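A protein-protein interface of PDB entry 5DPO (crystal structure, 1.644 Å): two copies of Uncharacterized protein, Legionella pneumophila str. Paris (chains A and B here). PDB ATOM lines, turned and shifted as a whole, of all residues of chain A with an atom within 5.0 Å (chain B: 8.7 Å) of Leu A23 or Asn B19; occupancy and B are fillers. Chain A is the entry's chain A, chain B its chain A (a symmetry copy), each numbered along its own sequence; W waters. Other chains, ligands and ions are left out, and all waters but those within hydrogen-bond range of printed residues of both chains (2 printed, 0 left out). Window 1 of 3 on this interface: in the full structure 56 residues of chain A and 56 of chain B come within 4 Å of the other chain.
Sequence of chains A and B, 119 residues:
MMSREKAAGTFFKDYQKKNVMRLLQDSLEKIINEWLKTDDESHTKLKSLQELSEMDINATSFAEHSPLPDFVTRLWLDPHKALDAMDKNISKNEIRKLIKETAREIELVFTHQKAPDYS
Of chain B, only Asn B19 and Val B20 come within 4 Å of Leu A23.
Printed residues of chain A within 4 Å of Phe B12: Ser A27 (3.8 Å).
Printed residues of chain B within 4 Å of Met A86: Gln B16 (3.3 Å).
Of the printed residues of chain A, Tyr B15 touches Asp A26.
Printed residues of chain B within 4 Å of Ser A27: Phe B12 (3.8 Å) and Gln B16 (3.3 Å).
Printed residues of chain A within 4 Å of Leu B98: Met A21.
Leu B83 touches none of the printed residues of chain A.
Gln A25 touches none of the printed residues of chain B.
Of the 11 printed residues of chain A, 7 touch a printed residue of chain B.
Printed residues of chain A that touch a printed residue of chain B: Asn A19, Val A20, Met A21, Leu A23, Asp A26, Ser A27 and Met A86.
Hydrophobic or aromatic side chains of chain A within 4 Å of the printed part of chain B: Met A21, Leu A23 and Met A86.
Hydrophobic or aromatic side chains of chain B that line the printed part of chain A: Phe B12, Tyr B15, Leu B23 and Leu B98.
Along chain B the printed residues that touch a printed residue of chain A span positions 12 to 98.
Among the printed residues, 11 pairs touch across the chains.
Among the printed residues, merely in contact across the chains: Asn A19 with Leu B23, Val A20 with Leu B23, Met A21 with Leu B98, Leu A23 with Asn B19, Leu A23 with Val B20, Ser A27 with Phe B12 and Met A86 with Gln B16.
Asn A19 touches Leu B23, and with the chains exchanged Leu A23 touches Asn B19.
Asn A19 touches Asp B26, and with the chains exchanged Asp A26 touches Asn B19.
Val A20 touches Leu B23, and with the chains exchanged Leu A23 touches Val B20.
9 positions are printed for both chains.
Water W1 lies within hydrogen-bond range of the side-chain amide nitrogen of Asn B19 (2.7 Å), the backbone carbonyl oxygen of Leu A23 (2.8 Å), the side-chain carboxylate of Asp A26 (2.9 Å) and the side-chain hydroxyl of Ser A27 (2.9 Å).
Water W2 lies within hydrogen-bond range of ND2 of Asn A19 (2.7 Å), O of Leu B23 (2.8 Å) and OD2 of Asp B26 (2.9 Å).
ND2 of Asn A19 lies within hydrogen-bond range of OD2 of Asp B26 (3.0 Å).
The side-chain hydroxyl (OH) of Tyr B15 lies close to the side-chain carboxylate (OD1) of Asp A26 (3.1 Å).
OD2 of Asp A26 sits at hydrogen-bond distance from ND2 of Asn B19, 3.0 Å away.
The side-chain amide nitrogen (NE2) of Gln B16 sits at hydrogen-bond distance from the side-chain hydroxyl (OG) of Ser A27 (3.3 Å).
OH of Tyr B15 lies close to ND2 of Asn B19, 3.4 Å away.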
ATOM      1  N   ASN A  19     -17.828  28.161  18.502  1.00  0.00           N
ATOM      2  CA  ASN A  19     -18.188  27.287  19.615  1.00  0.00           C
ATOM      3  C   ASN A  19     -17.852  27.892  20.976  1.00  0.00           C
ATOM      4  O   ASN A  19     -18.586  27.693  21.941  1.00  0.00           O
ATOM      5  CB  ASN A  19     -17.502  25.926  19.474  1.00  0.00           C
ATOM      6  CG  ASN A  19     -18.322  24.946  18.667  1.00  0.00           C
ATOM      7  OD1 ASN A  19     -19.357  25.301  18.107  1.00  0.00           O
ATOM      8  ND2 ASN A  19     -17.863  23.700  18.603  1.00  0.00           N
ATOM      9  N   VAL A  20     -16.745  28.625  21.050  1.00  0.00           N
ATOM     10  CA  VAL A  20     -16.377  29.308  22.285  1.00  0.00           C
ATOM     11  C   VAL A  20     -17.382  30.412  22.577  1.00  0.00           C
ATOM     12  O   VAL A  20     -17.805  30.590  23.719  1.00  0.00           O
ATOM     13  CB  VAL A  20     -14.949  29.901  22.216  1.00  0.00           C
ATOM     14  CG1 VAL A  20     -14.697  30.848  23.382  1.00  0.00           C
ATOM     15  CG2 VAL A  20     -13.917  28.785  22.204  1.00  0.00           C
ATOM     16  N   MET A  21     -17.774  31.139  21.533  1.00  0.00           N
ATOM     17  CA  MET A  21     -18.779  32.187  21.669  1.00  0.00           C
ATOM     18  C   MET A  21     -20.112  31.617  22.146  1.00  0.00           C
ATOM     19  O   MET A  21     -20.774  32.208  23.003  1.00  0.00           O
ATOM     20  CB  MET A  21     -18.962  32.928  20.341  1.00  0.00           C
ATOM     21  CG  MET A  21     -17.737  33.718  19.916  1.00  0.00           C
ATOM     22  SD  MET A  21     -17.270  35.138  21.171  1.00  0.00           S
ATOM     23  CE  MET A  21     -18.502  36.521  20.561  1.00  0.00           C
ATOM     24  N   ARG A  22     -20.507  30.488  21.610  1.00  0.00           N
ATOM     25  CA  ARG A  22     -21.698  29.771  22.069  1.00  0.00           C
ATOM     26  C   ARG A  22     -21.566  29.355  23.529  1.00  0.00           C
ATOM     27  O   ARG A  22     -22.528  29.425  24.290  1.00  0.00           O
ATOM     28  CB  ARG A  22     -21.958  28.527  21.213  1.00  0.00           C
ATOM     29  CG  ARG A  22     -22.326  28.782  19.769  1.00  0.00           C
ATOM     30  CD  ARG A  22     -22.628  27.464  19.063  1.00  0.00           C
ATOM     31  NE  ARG A  22     -22.969  27.646  17.656  1.00  0.00           N
ATOM     32  CZ  ARG A  22     -24.181  27.970  17.215  1.00  0.00           C
ATOM     33  NH1 ARG A  22     -25.177  28.148  18.073  1.00  0.00           N
ATOM     34  NH2 ARG A  22     -24.397  28.115  15.915  1.00  0.00           N
ATOM     35  N   LEU A  23     -20.452  28.882  23.891  1.00  0.00           N
ATOM     36  CA  LEU A  23     -20.227  28.470  25.273  1.00  0.00           C
ATOM     37  C   LEU A  23     -20.426  29.646  26.228  1.00  0.00           C
ATOM     38  O   LEU A  23     -21.064  29.519  27.273  1.00  0.00           O
ATOM     39  CB  LEU A  23     -18.819  27.886  25.433  1.00  0.00           C
ATOM     40  CG  LEU A  23     -18.383  27.518  26.851  1.00  0.00           C
ATOM     41  CD1 LEU A  23     -17.900  26.087  26.888  1.00  0.00           C
ATOM     42  CD2 LEU A  23     -17.291  28.457  27.320  1.00  0.00           C
ATOM     43  N   LEU A  24     -19.883  30.797  25.854  1.00  0.00           N
ATOM     44  CA  LEU A  24     -20.016  31.996  26.665  1.00  0.00           C
ATOM     45  C   LEU A  24     -21.469  32.470  26.708  1.00  0.00           C
ATOM     46  O   LEU A  24     -21.980  32.849  27.766  1.00  0.00           O
ATOM     47  CB  LEU A  24     -19.103  33.099  26.128  1.00  0.00           C
ATOM     48  CG  LEU A  24     -17.613  32.793  26.287  1.00  0.00           C
ATOM     49  CD1 LEU A  24     -16.758  33.857  25.629  1.00  0.00           C
ATOM     50  CD2 LEU A  24     -17.246  32.638  27.761  1.00  0.00           C
ATOM     51  N   GLN A  25     -22.137  32.441  25.561  1.00  0.00           N
ATOM     52  CA  GLN A  25     -23.530  32.865  25.511  1.00  0.00           C
ATOM     53  C   GLN A  25     -24.381  31.952  26.398  1.00  0.00           C
ATOM     54  O   GLN A  25     -25.260  32.421  27.119  1.00  0.00           O
ATOM     55  CB  GLN A  25     -24.049  32.866  24.073  1.00  0.00           C
ATOM     56  CG  GLN A  25     -25.508  33.265  23.947  1.00  0.00           C
ATOM     57  CD  GLN A  25     -26.001  33.238  22.516  1.00  0.00           C
ATOM     58  OE1 GLN A  25     -25.211  33.281  21.575  1.00  0.00           O
ATOM     59  NE2 GLN A  25     -27.315  33.170  22.345  1.00  0.00           N
ATOM     60  N   ASP A  26     -24.098  30.652  26.355  1.00  0.00           N
ATOM     61  CA  ASP A  26     -24.836  29.699  27.173  1.00  0.00           C
ATOM     62  C   ASP A  26     -24.665  29.988  28.666  1.00  0.00           C
ATOM     63  O   ASP A  26     -25.640  29.952  29.419  1.00  0.00           O
ATOM     64  CB  ASP A  26     -24.395  28.272  26.860  1.00  0.00           C
ATOM     65  CG  ASP A  26     -25.075  27.251  27.744  1.00  0.00           C
ATOM     66  OD1 ASP A  26     -26.242  26.902  27.462  1.00  0.00           O
ATOM     67  OD2 ASP A  26     -24.447  26.804  28.724  1.00  0.00           O
ATOM     68  N   SER A  27     -23.438  30.277  29.083  1.00  0.00           N
ATOM     69  CA  SER A  27     -23.156  30.594  30.475  1.00  0.00           C
ATOM     70  C   SER A  27     -23.833  31.888  30.906  1.00  0.00           C
ATOM     71  O   SER A  27     -24.373  31.970  32.011  1.00  0.00           O
ATOM     72  CB  SER A  27     -21.652  30.694  30.702  1.00  0.00           C
ATOM     73  OG  SER A  27     -21.128  29.427  31.043  1.00  0.00           O
ATOM     74  N   LEU A  83     -12.074  33.606  30.685  1.00  0.00           N
ATOM     75  CA  LEU A  83     -11.978  32.343  29.963  1.00  0.00           C
ATOM     76  C   LEU A  83     -10.886  31.436  30.532  1.00  0.00           C
ATOM     77  O   LEU A  83     -10.701  30.317  30.061  1.00  0.00           O
ATOM     78  CB  LEU A  83     -11.720  32.602  28.478  1.00  0.00           C
ATOM     79  CG  LEU A  83     -12.942  32.806  27.577  1.00  0.00           C
ATOM     80  CD1 LEU A  83     -12.550  33.492  26.276  1.00  0.00           C
ATOM     81  CD2 LEU A  83     -13.629  31.476  27.306  1.00  0.00           C
ATOM     82  N   MET A  86     -12.431  29.613  33.836  1.00  0.00           N
ATOM     83  CA  MET A  86     -13.415  28.636  33.396  1.00  0.00           C
ATOM     84  C   MET A  86     -12.823  27.234  33.284  1.00  0.00           C
ATOM     85  O   MET A  86     -13.541  26.241  33.407  1.00  0.00           O
ATOM     86  CB  MET A  86     -14.006  29.067  32.056  1.00  0.00           C
ATOM     87  CG  MET A  86     -15.492  28.824  31.921  1.00  0.00           C
ATOM     88  SD  MET A  86     -16.228  29.851  30.441  1.00  0.00           S
ATOM     89  CE  MET A  86     -18.111  29.615  30.817  1.00  0.00           C
ATOM     90  N   PHE B  12     -22.812  25.765  39.177  1.00  0.00           N
ATOM     91  CA  PHE B  12     -22.519  26.482  37.968  1.00  0.00           C
ATOM     92  C   PHE B  12     -21.099  26.203  37.504  1.00  0.00           C
ATOM     93  O   PHE B  12     -20.853  26.051  36.343  1.00  0.00           O
ATOM     94  CB  PHE B  12     -22.648  27.931  38.171  1.00  0.00           C
ATOM     95  CG  PHE B  12     -22.478  28.707  36.922  1.00  0.00           C
ATOM     96  CD1 PHE B  12     -21.671  29.791  36.889  1.00  0.00           C
ATOM     97  CD2 PHE B  12     -23.168  28.368  35.819  1.00  0.00           C
ATOM     98  CE1 PHE B  12     -21.531  30.531  35.739  1.00  0.00           C
ATOM     99  CE2 PHE B  12     -23.033  29.067  34.650  1.00  0.00           C
ATOM    100  CZ  PHE B  12     -22.212  30.167  34.614  1.00  0.00           C
ATOM    101  N   LYS B  13     -20.159  26.139  38.411  1.00  0.00           N
ATOM    102  CA  LYS B  13     -18.795  25.923  37.938  1.00  0.00           C
ATOM    103  C   LYS B  13     -18.616  24.507  37.404  1.00  0.00           C
ATOM    104  O   LYS B  13     -17.902  24.294  36.424  1.00  0.00           O
ATOM    105  CB  LYS B  13     -17.783  26.204  39.051  1.00  0.00           C
ATOM    106  CG  LYS B  13     -17.707  27.673  39.444  1.00  0.00           C
ATOM    107  CD  LYS B  13     -16.546  27.944  40.388  1.00  0.00           C
ATOM    108  CE  LYS B  13     -16.768  27.297  41.745  1.00  0.00           C
ATOM    109  NZ  LYS B  13     -15.696  27.655  42.714  1.00  0.00           N
ATOM    110  N   ASP B  14     -19.300  23.625  38.020  1.00  0.00           N
ATOM    111  CA  ASP B  14     -19.289  22.277  37.466  1.00  0.00           C
ATOM    112  C   ASP B  14     -19.920  22.287  36.080  1.00  0.00           C
ATOM    113  O   ASP B  14     -19.480  21.581  35.175  1.00  0.00           O
ATOM    114  CB  ASP B  14     -20.034  21.297  38.376  1.00  0.00           C
ATOM    115  CG  ASP B  14     -19.746  21.529  39.844  1.00  0.00           C
ATOM    116  OD1 ASP B  14     -19.732  22.704  40.273  1.00  0.00           O
ATOM    117  OD2 ASP B  14     -19.529  20.537  40.571  1.00  0.00           O
ATOM    118  N   TYR B  15     -20.964  23.094  35.926  1.00  0.00           N
ATOM    119  CA  TYR B  15     -21.652  23.219  34.647  1.00  0.00           C
ATOM    120  C   TYR B  15     -20.703  23.744  33.582  1.00  0.00           C
ATOM    121  O   TYR B  15     -20.635  23.216  32.467  1.00  0.00           O
ATOM    122  CB  TYR B  15     -22.851  24.150  34.775  1.00  0.00           C
ATOM    123  CG  TYR B  15     -23.549  24.415  33.470  1.00  0.00           C
ATOM    124  CD1 TYR B  15     -24.375  23.457  32.900  1.00  0.00           C
ATOM    125  CD2 TYR B  15     -23.378  25.620  32.801  1.00  0.00           C
ATOM    126  CE1 TYR B  15     -25.017  23.693  31.705  1.00  0.00           C
ATOM    127  CE2 TYR B  15     -24.016  25.863  31.606  1.00  0.00           C
ATOM    128  CZ  TYR B  15     -24.836  24.897  31.063  1.00  0.00           C
ATOM    129  OH  TYR B  15     -25.476  25.134  29.869  1.00  0.00           O
ATOM    130  N   GLN B  16     -19.961  24.783  33.944  1.00  0.00           N
ATOM    131  CA  GLN B  16     -19.009  25.394  33.028  1.00  0.00           C
ATOM    132  C   GLN B  16     -17.892  24.432  32.660  1.00  0.00           C
ATOM    133  O   GLN B  16     -17.505  24.357  31.495  1.00  0.00           O
ATOM    134  CB  GLN B  16     -18.439  26.673  33.639  1.00  0.00           C
ATOM    135  CG  GLN B  16     -19.463  27.797  33.702  1.00  0.00           C
ATOM    136  CD  GLN B  16     -18.887  29.094  34.229  1.00  0.00           C
ATOM    137  OE1 GLN B  16     -17.944  29.095  35.018  1.00  0.00           O
ATOM    138  NE2 GLN B  16     -19.454  30.211  33.790  1.00  0.00           N
ATOM    139  N   LYS B  17     -17.393  23.688  33.645  1.00  0.00           N
ATOM    140  CA  LYS B  17     -16.356  22.690  33.396  1.00  0.00           C
ATOM    141  C   LYS B  17     -16.822  21.636  32.400  1.00  0.00           C
ATOM    142  O   LYS B  17     -16.120  21.325  31.439  1.00  0.00           O
ATOM    143  CB  LYS B  17     -15.923  22.012  34.700  1.00  0.00           C
ATOM    144  CG  LYS B  17     -14.886  20.909  34.492  1.00  0.00           C
ATOM    145  CD  LYS B  17     -14.333  20.392  35.810  1.00  0.00           C
ATOM    146  CE  LYS B  17     -13.478  19.155  35.581  1.00  0.00           C
ATOM    147  NZ  LYS B  17     -13.018  18.530  36.849  1.00  0.00           N
ATOM    148  N   LYS B  18     -18.011  21.090  32.632  1.00  0.00           N
ATOM    149  CA  LYS B  18     -18.540  20.054  31.761  1.00  0.00           C
ATOM    150  C   LYS B  18     -18.728  20.576  30.341  1.00  0.00           C
ATOM    151  O   LYS B  18     -18.495  19.852  29.377  1.00  0.00           O
ATOM    152  CB  LYS B  18     -19.855  19.506  32.321  1.00  0.00           C
ATOM    153  CG  LYS B  18     -19.669  18.789  33.652  1.00  0.00           C
ATOM    154  CD  LYS B  18     -20.955  18.176  34.182  1.00  0.00           C
ATOM    155  CE  LYS B  18     -20.701  17.471  35.510  1.00  0.00           C
ATOM    156  NZ  LYS B  18     -21.918  16.815  36.063  1.00  0.00           N
ATOM    157  N   ASN B  19     -19.125  21.838  30.218  1.00  0.00           N
ATOM    158  CA  ASN B  19     -19.302  22.449  28.903  1.00  0.00           C
ATOM    159  C   ASN B  19     -17.982  22.658  28.164  1.00  0.00           C
ATOM    160  O   ASN B  19     -17.927  22.524  26.944  1.00  0.00           O
ATOM    161  CB  ASN B  19     -20.039  23.786  29.024  1.00  0.00           C
ATOM    162  CG  ASN B  19     -21.541  23.625  28.959  1.00  0.00           C
ATOM    163  OD1 ASN B  19     -22.056  22.509  28.937  1.00  0.00           O
ATOM    164  ND2 ASN B  19     -22.256  24.745  28.927  1.00  0.00           N
ATOM    165  N   VAL B  20     -16.926  22.987  28.902  1.00  0.00           N
ATOM    166  CA  VAL B  20     -15.606  23.134  28.302  1.00  0.00           C
ATOM    167  C   VAL B  20     -15.112  21.778  27.819  1.00  0.00           C
ATOM    168  O   VAL B  20     -14.553  21.666  26.728  1.00  0.00           O
ATOM    169  CB  VAL B  20     -14.584  23.744  29.291  1.00  0.00           C
ATOM    170  CG1 VAL B  20     -13.165  23.617  28.754  1.00  0.00           C
ATOM    171  CG2 VAL B  20     -14.922  25.199  29.565  1.00  0.00           C
ATOM    172  N   MET B  21     -15.338  20.748  28.630  1.00  0.00           N
ATOM    173  CA  MET B  21     -14.968  19.388  28.255  1.00  0.00           C
ATOM    174  C   MET B  21     -15.709  18.939  27.000  1.00  0.00           C
ATOM    175  O   MET B  21     -15.119  18.313  26.115  1.00  0.00           O
ATOM    176  CB  MET B  21     -15.245  18.420  29.410  1.00  0.00           C
ATOM    177  CG  MET B  21     -14.368  18.664  30.625  1.00  0.00           C
ATOM    178  SD  MET B  21     -12.468  18.406  30.259  1.00  0.00           S
ATOM    179  CE  MET B  21     -12.367  16.467  30.445  1.00  0.00           C
ATOM    180  N   ARG B  22     -16.980  19.251  26.909  1.00  0.00           N
ATOM    181  CA  ARG B  22     -17.771  18.993  25.706  1.00  0.00           C
ATOM    182  C   ARG B  22     -17.214  19.747  24.504  1.00  0.00           C
ATOM    183  O   ARG B  22     -17.181  19.223  23.394  1.00  0.00           O
ATOM    184  CB  ARG B  22     -19.237  19.391  25.912  1.00  0.00           C
ATOM    185  CG  ARG B  22     -20.005  18.577  26.929  1.00  0.00           C
ATOM    186  CD  ARG B  22     -21.460  19.031  26.975  1.00  0.00           C
ATOM    187  NE  ARG B  22     -22.248  18.296  27.958  1.00  0.00           N
ATOM    188  CZ  ARG B  22     -22.799  17.106  27.737  1.00  0.00           C
ATOM    189  NH1 ARG B  22     -22.651  16.512  26.560  1.00  0.00           N
ATOM    190  NH2 ARG B  22     -23.499  16.511  28.693  1.00  0.00           N
ATOM    191  N   LEU B  23     -16.856  20.944  24.696  1.00  0.00           N
ATOM    192  CA  LEU B  23     -16.296  21.741  23.608  1.00  0.00           C
ATOM    193  C   LEU B  23     -15.031  21.089  23.054  1.00  0.00           C
ATOM    194  O   LEU B  23     -14.838  20.997  21.842  1.00  0.00           O
ATOM    195  CB  LEU B  23     -15.996  23.165  24.090  1.00  0.00           C
ATOM    196  CG  LEU B  23     -15.291  24.093  23.101  1.00  0.00           C
ATOM    197  CD1 LEU B  23     -16.072  25.377  22.952  1.00  0.00           C
ATOM    198  CD2 LEU B  23     -13.881  24.382  23.572  1.00  0.00           C
ATOM    199  N   LEU B  24     -14.174  20.626  23.954  1.00  0.00           N
ATOM    200  CA  LEU B  24     -12.940  19.966  23.556  1.00  0.00           C
ATOM    201  C   LEU B  24     -13.230  18.637  22.859  1.00  0.00           C
ATOM    202  O   LEU B  24     -12.613  18.310  21.841  1.00  0.00           O
ATOM    203  CB  LEU B  24     -12.041  19.755  24.775  1.00  0.00           C
ATOM    204  CG  LEU B  24     -11.507  21.055  25.376  1.00  0.00           C
ATOM    205  CD1 LEU B  24     -10.726  20.794  26.648  1.00  0.00           C
ATOM    206  CD2 LEU B  24     -10.651  21.810  24.362  1.00  0.00           C
ATOM    207  N   GLN B  25     -14.172  17.875  23.401  1.00  0.00           N
ATOM    208  CA  GLN B  25     -14.521  16.597  22.796  1.00  0.00           C
ATOM    209  C   GLN B  25     -15.067  16.823  21.384  1.00  0.00           C
ATOM    210  O   GLN B  25     -14.735  16.086  20.457  1.00  0.00           O
ATOM    211  CB  GLN B  25     -15.533  15.843  23.659  1.00  0.00           C
ATOM    212  CG  GLN B  25     -15.970  14.513  23.072  1.00  0.00           C
ATOM    213  CD  GLN B  25     -16.987  13.798  23.935  1.00  0.00           C
ATOM    214  OE1 GLN B  25     -17.116  14.080  25.125  1.00  0.00           O
ATOM    215  NE2 GLN B  25     -17.716  12.864  23.339  1.00  0.00           N
ATOM    216  N   ASP B  26     -15.887  17.859  21.225  1.00  0.00           N
ATOM    217  CA  ASP B  26     -16.450  18.174  19.919  1.00  0.00           C
ATOM    218  C   ASP B  26     -15.356  18.506  18.901  1.00  0.00           C
ATOM    219  O   ASP B  26     -15.408  18.037  17.762  1.00  0.00           O
ATOM    220  CB  ASP B  26     -17.437  19.333  20.026  1.00  0.00           C
ATOM    221  CG  ASP B  26     -17.985  19.750  18.681  1.00  0.00           C
ATOM    222  OD1 ASP B  26     -18.908  19.073  18.177  1.00  0.00           O
ATOM    223  OD2 ASP B  26     -17.490  20.748  18.123  1.00  0.00           O
ATOM    224  N   LEU B  83      -6.063  25.635  25.105  1.00  0.00           N
ATOM    225  CA  LEU B  83      -7.310  26.333  25.394  1.00  0.00           C
ATOM    226  C   LEU B  83      -7.157  27.851  25.294  1.00  0.00           C
ATOM    227  O   LEU B  83      -8.125  28.585  25.470  1.00  0.00           O
ATOM    228  CB  LEU B  83      -7.817  25.950  26.786  1.00  0.00           C
ATOM    229  CG  LEU B  83      -8.709  24.710  26.893  1.00  0.00           C
ATOM    230  CD1 LEU B  83      -8.754  24.194  28.324  1.00  0.00           C
ATOM    231  CD2 LEU B  83     -10.108  25.015  26.380  1.00  0.00           C
ATOM    232  N   LEU B  98     -21.280  40.700  22.509  1.00  0.00           N
ATOM    233  CA  LEU B  98     -22.050  39.496  22.810  1.00  0.00           C
ATOM    234  C   LEU B  98     -22.838  39.656  24.106  1.00  0.00           C
ATOM    235  O   LEU B  98     -24.006  39.267  24.192  1.00  0.00           O
ATOM    236  CB  LEU B  98     -21.128  38.274  22.907  1.00  0.00           C
ATOM    237  CG  LEU B  98     -21.782  36.984  23.407  1.00  0.00           C
ATOM    238  CD1 LEU B  98     -22.776  36.465  22.383  1.00  0.00           C
ATOM    239  CD2 LEU B  98     -20.720  35.926  23.709  1.00  0.00           C
HETATM  240  O   HOH W   1     -21.632  27.392  29.025  1.00  0.00           O
HETATM  241  O   HOH W   2     -15.651  22.446  19.571  1.00  0.00           O
